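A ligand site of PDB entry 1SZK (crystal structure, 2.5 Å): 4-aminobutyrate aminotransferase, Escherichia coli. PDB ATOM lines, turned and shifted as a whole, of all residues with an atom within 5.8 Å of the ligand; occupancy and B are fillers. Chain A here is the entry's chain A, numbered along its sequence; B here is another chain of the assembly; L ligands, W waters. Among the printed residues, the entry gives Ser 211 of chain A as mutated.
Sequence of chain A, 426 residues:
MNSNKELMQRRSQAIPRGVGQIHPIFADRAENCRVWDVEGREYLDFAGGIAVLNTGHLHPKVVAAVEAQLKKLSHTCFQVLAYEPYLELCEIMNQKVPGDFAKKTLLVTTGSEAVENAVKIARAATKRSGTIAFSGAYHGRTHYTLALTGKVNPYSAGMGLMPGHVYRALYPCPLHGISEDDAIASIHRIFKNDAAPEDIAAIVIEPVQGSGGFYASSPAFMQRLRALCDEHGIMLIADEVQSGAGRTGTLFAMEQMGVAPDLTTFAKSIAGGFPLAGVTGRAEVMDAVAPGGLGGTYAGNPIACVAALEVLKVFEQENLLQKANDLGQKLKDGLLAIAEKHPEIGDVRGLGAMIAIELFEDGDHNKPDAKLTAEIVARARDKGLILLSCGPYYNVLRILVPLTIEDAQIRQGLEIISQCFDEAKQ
An oxygen (O1) of the ligand lies within hydrogen-bond range of the side-chain amide nitrogen (NE2) of Gln 242, at 2.7 Å. N of Thr 297 of chain B sits at hydrogen-bond distance from O4 of the ligand (2.8 Å). O5 of the ligand is in hydrogen-bond range of OG of Ser 112 (2.8 Å). A nitrogen (N1) of the ligand sits at hydrogen-bond distance from the side-chain carboxylate of Asp 239, at 2.7 Å. An oxygen (O5) of the ligand lies within hydrogen-bond range of the backbone NH (N) of Ser 112, at 3.0 Å. The side-chain hydroxyl (OG1) of Thr 297 of chain B lies within hydrogen-bond range of an oxygen (O4) of the ligand, 2.6 Å away. N of Gly 111 sits at hydrogen-bond distance from O3 of the ligand (2.9 Å).
The side-chain hydroxyl (OG1) of Thr 297 of chain B sits at hydrogen-bond distance from the side-chain amino group (NZ) of Lys 268 (2.9 Å). The side-chain hydroxyl of Thr 110 lies within hydrogen-bond range of the backbone NH of Glu 113 of chain A, at 3.3 Å. The side-chain carboxylate of Asp 239 lies within hydrogen-bond range of the backbone NH of Val 241. OD2 of Asp 239 is in hydrogen-bond range of ND1 of His 139 (2.8 Å). OE1 of Glu 206 lies within hydrogen-bond range of N of Tyr 138. The side-chain hydroxyl (OG) of Ser 112 sits at hydrogen-bond distance from the backbone NH (N) of Arg 141 (3.3 Å). NZ of Lys 268 sits at hydrogen-bond distance from O of Ile 50 (3.3 Å). The backbone NH (N) of Lys 268 lies within hydrogen-bond range of the side-chain hydroxyl (OH) of Tyr 298 of chain B (2.7 Å).
A nitrogen (N1) of the ligand lies close to the backbone carbonyl oxygen (O) of Tyr 138, 3.3 Å away. Thr 110 touches the ligand. His 139 touches the ligand (O to C7, 3.4 Å). CA of Gly 140 touches C8 of the ligand, at 3.98 Å. Glu 206 touches the ligand. Val 241 touches the ligand. Lys 268 touches the ligand. Gly 296 of chain B touches the ligand (CA to O4, 3.7 Å). 13 residues have an atom within 4 Å of the ligand: Thr 110, Gly 111, Ser 112, Tyr 138, His 139, Gly 140, Glu 206, Asp 239, Val 241, Gln 242, Lys 268, Gly 296 of chain B and Thr 297 of chain B. The nearest printed residue that does not touch the ligand is Tyr 298 of chain B (4.4 Å).
Water W7 lies within hydrogen-bond range of O5 of the ligand (2.5 Å) and OE2 of Glu 113 of chain B (2.6 Å). Water W4 lies within hydrogen-bond range of an oxygen (O3) of the ligand (2.6 Å), the backbone NH (N) of Tyr 298 of chain B (2.7 Å) and the backbone NH (N) of Thr 297 of chain B (3.4 Å). Water W1 lies within hydrogen-bond range of an oxygen (O4) of the ligand (2.7 Å) and the side-chain hydroxyl of Tyr 138 (2.7 Å). Water W2 lies within hydrogen-bond range of O1 of the ligand, OE2 of Glu 206, N of Ser 211 and NE2 of Gln 242. Water W3 bridges an oxygen (O3) of the ligand (2.8 Å) and the backbone NH (N) of Lys 268 (3.1 Å). Water W5 lies within hydrogen-bond range of OE2 of Glu 206 (2.7 Å) and N of Gly 210 (3.2 Å).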
ATOM      1  N   ILE A  50       4.624  22.381  12.083  1.00  0.00           N
ATOM      2  CA  ILE A  50       5.521  22.838  11.026  1.00  0.00           C
ATOM      3  C   ILE A  50       5.770  24.345  11.112  1.00  0.00           C
ATOM      4  O   ILE A  50       5.395  25.111  10.217  1.00  0.00           O
ATOM      5  CB  ILE A  50       5.026  22.488   9.595  1.00  0.00           C
ATOM      6  CG1 ILE A  50       4.485  21.058   9.539  1.00  0.00           C
ATOM      7  CG2 ILE A  50       6.195  22.582   8.622  1.00  0.00           C
ATOM      8  CD1 ILE A  50       4.066  20.603   8.153  1.00  0.00           C
ATOM      9  N   THR A 110      -3.401  31.724   3.372  1.00  0.00           N
ATOM     10  CA  THR A 110      -2.359  30.687   3.457  1.00  0.00           C
ATOM     11  C   THR A 110      -1.022  31.160   2.901  1.00  0.00           C
ATOM     12  O   THR A 110      -0.948  32.157   2.182  1.00  0.00           O
ATOM     13  CB  THR A 110      -2.762  29.397   2.689  1.00  0.00           C
ATOM     14  OG1 THR A 110      -2.728  29.661   1.283  1.00  0.00           O
ATOM     15  CG2 THR A 110      -4.166  28.938   3.079  1.00  0.00           C
ATOM     16  N   GLY A 111       0.020  30.411   3.235  1.00  0.00           N
ATOM     17  CA  GLY A 111       1.357  30.735   2.753  1.00  0.00           C
ATOM     18  C   GLY A 111       1.445  30.719   1.239  1.00  0.00           C
ATOM     19  O   GLY A 111       2.093  31.584   0.641  1.00  0.00           O
ATOM     20  N   SER A 112       0.789  29.738   0.611  1.00  0.00           N
ATOM     21  CA  SER A 112       0.821  29.643  -0.846  1.00  0.00           C
ATOM     22  C   SER A 112       0.171  30.873  -1.466  1.00  0.00           C
ATOM     23  O   SER A 112       0.666  31.388  -2.481  1.00  0.00           O
ATOM     24  CB  SER A 112       0.090  28.370  -1.309  1.00  0.00           C
ATOM     25  OG  SER A 112       0.763  27.209  -0.844  1.00  0.00           O
ATOM     26  N   GLU A 113      -0.923  31.345  -0.877  1.00  0.00           N
ATOM     27  CA  GLU A 113      -1.596  32.514  -1.384  1.00  0.00           C
ATOM     28  C   GLU A 113      -0.650  33.710  -1.231  1.00  0.00           C
ATOM     29  O   GLU A 113      -0.558  34.562  -2.107  1.00  0.00           O
ATOM     30  CB  GLU A 113      -2.889  32.768  -0.618  1.00  0.00           C
ATOM     31  CG  GLU A 113      -3.981  31.754  -0.917  1.00  0.00           C
ATOM     32  CD  GLU A 113      -5.332  32.210  -0.395  1.00  0.00           C
ATOM     33  OE1 GLU A 113      -5.386  32.750   0.741  1.00  0.00           O
ATOM     34  OE2 GLU A 113      -6.346  32.035  -1.112  1.00  0.00           O
ATOM     35  N   VAL A 115       2.600  33.756  -1.327  1.00  0.00           N
ATOM     36  CA  VAL A 115       3.539  33.734  -2.446  1.00  0.00           C
ATOM     37  C   VAL A 115       2.838  34.038  -3.770  1.00  0.00           C
ATOM     38  O   VAL A 115       3.381  34.726  -4.617  1.00  0.00           O
ATOM     39  CB  VAL A 115       4.295  32.394  -2.541  1.00  0.00           C
ATOM     40  CG1 VAL A 115       5.160  32.389  -3.788  1.00  0.00           C
ATOM     41  CG2 VAL A 115       5.168  32.195  -1.307  1.00  0.00           C
ATOM     42  N   TYR A 138      10.823  25.616  -1.370  1.00  0.00           N
ATOM     43  CA  TYR A 138       9.444  25.201  -1.215  1.00  0.00           C
ATOM     44  C   TYR A 138       8.583  26.463  -1.030  1.00  0.00           C
ATOM     45  O   TYR A 138       8.776  27.232  -0.092  1.00  0.00           O
ATOM     46  CB  TYR A 138       9.265  24.291  -0.013  1.00  0.00           C
ATOM     47  CG  TYR A 138       7.857  23.787   0.104  1.00  0.00           C
ATOM     48  CD1 TYR A 138       7.471  22.576  -0.474  1.00  0.00           C
ATOM     49  CD2 TYR A 138       6.889  24.535   0.774  1.00  0.00           C
ATOM     50  CE1 TYR A 138       6.151  22.125  -0.386  1.00  0.00           C
ATOM     51  CE2 TYR A 138       5.573  24.105   0.861  1.00  0.00           C
ATOM     52  CZ  TYR A 138       5.208  22.899   0.287  1.00  0.00           C
ATOM     53  OH  TYR A 138       3.913  22.456   0.409  1.00  0.00           O
ATOM     54  N   HIS A 139       7.632  26.675  -1.923  1.00  0.00           N
ATOM     55  CA  HIS A 139       6.804  27.864  -1.858  1.00  0.00           C
ATOM     56  C   HIS A 139       5.299  27.638  -1.835  1.00  0.00           C
ATOM     57  O   HIS A 139       4.550  28.606  -1.797  1.00  0.00           O
ATOM     58  CB  HIS A 139       7.171  28.782  -3.015  1.00  0.00           C
ATOM     59  CG  HIS A 139       8.623  29.170  -3.042  1.00  0.00           C
ATOM     60  ND1 HIS A 139       9.193  29.980  -2.087  1.00  0.00           N
ATOM     61  CD2 HIS A 139       9.611  28.846  -3.899  1.00  0.00           C
ATOM     62  CE1 HIS A 139      10.477  30.142  -2.350  1.00  0.00           C
ATOM     63  NE2 HIS A 139      10.755  29.461  -3.442  1.00  0.00           N
ATOM     64  N   GLY A 140       4.863  26.373  -1.866  1.00  0.00           N
ATOM     65  CA  GLY A 140       3.432  26.093  -1.845  1.00  0.00           C
ATOM     66  C   GLY A 140       2.951  24.992  -2.777  1.00  0.00           C
ATOM     67  O   GLY A 140       3.708  24.499  -3.612  1.00  0.00           O
ATOM     68  N   ARG A 141       1.675  24.636  -2.669  1.00  0.00           N
ATOM     69  CA  ARG A 141       1.110  23.558  -3.476  1.00  0.00           C
ATOM     70  C   ARG A 141       0.139  23.925  -4.590  1.00  0.00           C
ATOM     71  O   ARG A 141      -0.479  23.031  -5.179  1.00  0.00           O
ATOM     72  CB  ARG A 141       0.441  22.531  -2.560  1.00  0.00           C
ATOM     73  CG  ARG A 141       1.425  21.782  -1.685  1.00  0.00           C
ATOM     74  CD  ARG A 141       0.701  20.966  -0.624  1.00  0.00           C
ATOM     75  NE  ARG A 141       1.640  20.170   0.175  1.00  0.00           N
ATOM     76  CZ  ARG A 141       2.175  19.010  -0.203  1.00  0.00           C
ATOM     77  NH1 ARG A 141       1.868  18.484  -1.388  1.00  0.00           N
ATOM     78  NH2 ARG A 141       3.022  18.395   0.594  1.00  0.00           N
ATOM     79  N   GLU A 206      14.074  31.836   0.015  1.00  0.00           N
ATOM     80  CA  GLU A 206      13.864  31.585   1.438  1.00  0.00           C
ATOM     81  C   GLU A 206      15.158  32.031   2.132  1.00  0.00           C
ATOM     82  O   GLU A 206      16.214  31.501   1.827  1.00  0.00           O
ATOM     83  CB  GLU A 206      13.652  30.089   1.685  1.00  0.00           C
ATOM     84  CG  GLU A 206      12.214  29.614   1.467  1.00  0.00           C
ATOM     85  CD  GLU A 206      12.129  28.136   1.164  1.00  0.00           C
ATOM     86  OE1 GLU A 206      12.393  27.759   0.001  1.00  0.00           O
ATOM     87  OE2 GLU A 206      11.802  27.351   2.082  1.00  0.00           O
ATOM     88  N   GLY A 210      13.353  25.892   4.435  1.00  0.00           N
ATOM     89  CA  GLY A 210      12.747  25.052   5.458  1.00  0.00           C
ATOM     90  C   GLY A 210      12.710  23.619   5.007  1.00  0.00           C
ATOM     91  O   GLY A 210      13.509  22.800   5.455  1.00  0.00           O
ATOM     92  N   SER A 211      11.771  23.319   4.121  1.00  0.00           N
ATOM     93  CA  SER A 211      11.622  21.992   3.548  1.00  0.00           C
ATOM     94  C   SER A 211      12.941  21.596   2.882  1.00  0.00           C
ATOM     95  O   SER A 211      13.334  20.433   2.896  1.00  0.00           O
ATOM     96  CB  SER A 211      10.492  22.016   2.505  1.00  0.00           C
ATOM     97  OG  SER A 211      10.647  20.996   1.522  1.00  0.00           O
ATOM     98  N   ASP A 239      10.590  34.802   0.932  1.00  0.00           N
ATOM     99  CA  ASP A 239       9.527  33.960   1.451  1.00  0.00           C
ATOM    100  C   ASP A 239       9.898  33.621   2.889  1.00  0.00           C
ATOM    101  O   ASP A 239      10.779  32.786   3.130  1.00  0.00           O
ATOM    102  CB  ASP A 239       9.394  32.696   0.599  1.00  0.00           C
ATOM    103  CG  ASP A 239       8.240  31.814   1.022  1.00  0.00           C
ATOM    104  OD1 ASP A 239       7.581  32.096   2.058  1.00  0.00           O
ATOM    105  OD2 ASP A 239       7.976  30.808   0.327  1.00  0.00           O
ATOM    106  N   GLU A 240       9.238  34.276   3.850  1.00  0.00           N
ATOM    107  CA  GLU A 240       9.500  34.058   5.268  1.00  0.00           C
ATOM    108  C   GLU A 240       8.318  33.401   5.972  1.00  0.00           C
ATOM    109  O   GLU A 240       8.103  33.568   7.173  1.00  0.00           O
ATOM    110  CB  GLU A 240       9.858  35.374   5.973  1.00  0.00           C
ATOM    111  CG  GLU A 240      11.140  35.989   5.404  1.00  0.00           C
ATOM    112  CD  GLU A 240      12.122  36.403   6.482  1.00  0.00           C
ATOM    113  OE1 GLU A 240      12.314  35.603   7.437  1.00  0.00           O
ATOM    114  OE2 GLU A 240      12.703  37.510   6.370  1.00  0.00           O
ATOM    115  N   VAL A 241       7.568  32.644   5.183  1.00  0.00           N
ATOM    116  CA  VAL A 241       6.424  31.908   5.687  1.00  0.00           C
ATOM    117  C   VAL A 241       6.878  30.998   6.835  1.00  0.00           C
ATOM    118  O   VAL A 241       6.172  30.869   7.847  1.00  0.00           O
ATOM    119  CB  VAL A 241       5.808  31.046   4.555  1.00  0.00           C
ATOM    120  CG1 VAL A 241       5.045  29.855   5.131  1.00  0.00           C
ATOM    121  CG2 VAL A 241       4.872  31.930   3.717  1.00  0.00           C
ATOM    122  N   GLN A 242       8.057  30.401   6.681  1.00  0.00           N
ATOM    123  CA  GLN A 242       8.579  29.503   7.707  1.00  0.00           C
ATOM    124  C   GLN A 242       9.731  30.094   8.515  1.00  0.00           C
ATOM    125  O   GLN A 242       9.849  29.851   9.703  1.00  0.00           O
ATOM    126  CB  GLN A 242       9.031  28.161   7.075  1.00  0.00           C
ATOM    127  CG  GLN A 242       9.575  27.135   8.086  1.00  0.00           C
ATOM    128  CD  GLN A 242       9.687  25.708   7.519  1.00  0.00           C
ATOM    129  OE1 GLN A 242      10.164  24.789   8.192  1.00  0.00           O
ATOM    130  NE2 GLN A 242       9.236  25.532   6.276  1.00  0.00           N
ATOM    131  N   SER A 243      10.582  30.878   7.870  1.00  0.00           N
ATOM    132  CA  SER A 243      11.705  31.479   8.569  1.00  0.00           C
ATOM    133  C   SER A 243      11.265  32.656   9.413  1.00  0.00           C
ATOM    134  O   SER A 243      11.993  33.096  10.287  1.00  0.00           O
ATOM    135  CB  SER A 243      12.732  31.965   7.565  1.00  0.00           C
ATOM    136  OG  SER A 243      12.149  32.959   6.764  1.00  0.00           O
ATOM    137  N   ALA A 267       3.294  33.733   7.274  1.00  0.00           N
ATOM    138  CA  ALA A 267       2.157  32.887   7.646  1.00  0.00           C
ATOM    139  C   ALA A 267       2.559  32.040   8.849  1.00  0.00           C
ATOM    140  O   ALA A 267       3.364  32.475   9.698  1.00  0.00           O
ATOM    141  CB  ALA A 267       1.767  31.981   6.489  1.00  0.00           C
ATOM    142  N   LYS A 268       2.009  30.833   8.925  1.00  0.00           N
ATOM    143  CA  LYS A 268       2.296  29.890  10.003  1.00  0.00           C
ATOM    144  C   LYS A 268       2.265  30.511  11.402  1.00  0.00           C
ATOM    145  O   LYS A 268       1.201  30.842  11.928  1.00  0.00           O
ATOM    146  CB  LYS A 268       3.652  29.226   9.787  1.00  0.00           C
ATOM    147  CG  LYS A 268       3.806  28.486   8.493  1.00  0.00           C
ATOM    148  CD  LYS A 268       5.180  27.857   8.419  1.00  0.00           C
ATOM    149  CE  LYS A 268       5.338  26.976   7.190  1.00  0.00           C
ATOM    150  NZ  LYS A 268       4.367  25.845   7.210  1.00  0.00           N
ATOM    151  N   GLU B 113      -7.795  27.278  -3.310  1.00  0.00           N
ATOM    152  CA  GLU B 113      -7.018  26.064  -3.096  1.00  0.00           C
ATOM    153  C   GLU B 113      -7.833  24.868  -3.541  1.00  0.00           C
ATOM    154  O   GLU B 113      -7.302  23.940  -4.155  1.00  0.00           O
ATOM    155  CB  GLU B 113      -6.663  25.903  -1.625  1.00  0.00           C
ATOM    156  CG  GLU B 113      -5.548  26.829  -1.161  1.00  0.00           C
ATOM    157  CD  GLU B 113      -5.083  26.501   0.233  1.00  0.00           C
ATOM    158  OE1 GLU B 113      -5.936  26.364   1.147  1.00  0.00           O
ATOM    159  OE2 GLU B 113      -3.852  26.372   0.435  1.00  0.00           O
ATOM    160  N   GLY B 295      -1.204  18.585   0.353  1.00  0.00           N
ATOM    161  CA  GLY B 295      -0.937  19.185   1.647  1.00  0.00           C
ATOM    162  C   GLY B 295      -1.424  20.611   1.816  1.00  0.00           C
ATOM    163  O   GLY B 295      -2.297  21.102   1.087  1.00  0.00           O
ATOM    164  N   GLY B 296      -0.828  21.295   2.787  1.00  0.00           N
ATOM    165  CA  GLY B 296      -1.199  22.655   3.096  1.00  0.00           C
ATOM    166  C   GLY B 296      -1.218  22.821   4.599  1.00  0.00           C
ATOM    167  O   GLY B 296      -2.002  22.180   5.296  1.00  0.00           O
ATOM    168  N   THR B 297      -0.323  23.658   5.102  1.00  0.00           N
ATOM    169  CA  THR B 297      -0.208  23.907   6.531  1.00  0.00           C
ATOM    170  C   THR B 297      -1.532  24.005   7.315  1.00  0.00           C
ATOM    171  O   THR B 297      -1.774  23.202   8.210  1.00  0.00           O
ATOM    172  CB  THR B 297       0.581  25.199   6.779  1.00  0.00           C
ATOM    173  OG1 THR B 297       1.808  25.142   6.045  1.00  0.00           O
ATOM    174  CG2 THR B 297       0.883  25.355   8.273  1.00  0.00           C
ATOM    175  N   TYR B 298      -2.366  24.978   6.969  1.00  0.00           N
ATOM    176  CA  TYR B 298      -3.628  25.202   7.661  1.00  0.00           C
ATOM    177  C   TYR B 298      -4.776  24.274   7.252  1.00  0.00           C
ATOM    178  O   TYR B 298      -5.819  24.241   7.917  1.00  0.00           O
ATOM    179  CB  TYR B 298      -4.096  26.654   7.454  1.00  0.00           C
ATOM    180  CG  TYR B 298      -3.135  27.722   7.937  1.00  0.00           C
ATOM    181  CD1 TYR B 298      -2.619  27.696   9.242  1.00  0.00           C
ATOM    182  CD2 TYR B 298      -2.789  28.795   7.120  1.00  0.00           C
ATOM    183  CE1 TYR B 298      -1.791  28.707   9.717  1.00  0.00           C
ATOM    184  CE2 TYR B 298      -1.958  29.815   7.584  1.00  0.00           C
ATOM    185  CZ  TYR B 298      -1.466  29.763   8.887  1.00  0.00           C
ATOM    186  OH  TYR B 298      -0.687  30.793   9.361  1.00  0.00           O
HETATM  187  N1  LIG L   1       6.595  28.902   1.738  1.00  0.00           N
HETATM  188  C1  LIG L   1       7.445  28.272   2.660  1.00  0.00           C
HETATM  189  C2  LIG L   1       8.856  28.857   2.751  1.00  0.00           C
HETATM  190  C3  LIG L   1       6.897  27.104   3.468  1.00  0.00           C
HETATM  191  O1  LIG L   1       7.739  26.534   4.331  1.00  0.00           O
HETATM  192  C4  LIG L   1       5.596  26.657   3.314  1.00  0.00           C
HETATM  193  C5  LIG L   1       5.049  25.500   4.131  1.00  0.00           C
HETATM  194  N2  LIG L   1       4.740  24.152   3.560  1.00  0.00           N
HETATM  195  C6  LIG L   1       4.684  27.424   2.256  1.00  0.00           C
HETATM  196  C7  LIG L   1       5.237  28.483   1.530  1.00  0.00           C
HETATM  197  C8  LIG L   1       3.251  27.018   2.022  1.00  0.00           C
HETATM  198  O2  LIG L   1       2.419  27.535   3.045  1.00  0.00           O
HETATM  199  P1  LIG L   1       0.982  26.958   3.194  1.00  0.00           P
HETATM  200  O3  LIG L   1       0.420  27.747   4.345  1.00  0.00           O
HETATM  201  O4  LIG L   1       1.111  25.505   3.532  1.00  0.00           O
HETATM  202  O5  LIG L   1       0.228  27.132   1.913  1.00  0.00           O
HETATM  203  O   HOH W   1       1.933  23.600   1.865  1.00  0.00           O
HETATM  204  O   HOH W   2      10.028  25.584   3.202  1.00  0.00           O
HETATM  205  O   HOH W   3       1.082  28.706   6.856  1.00  0.00           O
HETATM  206  O   HOH W   4      -1.878  26.629   4.891  1.00  0.00           O
HETATM  207  O   HOH W   5      11.882  28.727   4.456  1.00  0.00           O
HETATM  208  O   HOH W   6       0.576  24.885   0.187  1.00  0.00           O
HETATM  209  O   HOH W   7      -1.942  26.016   2.186  1.00  0.00           O
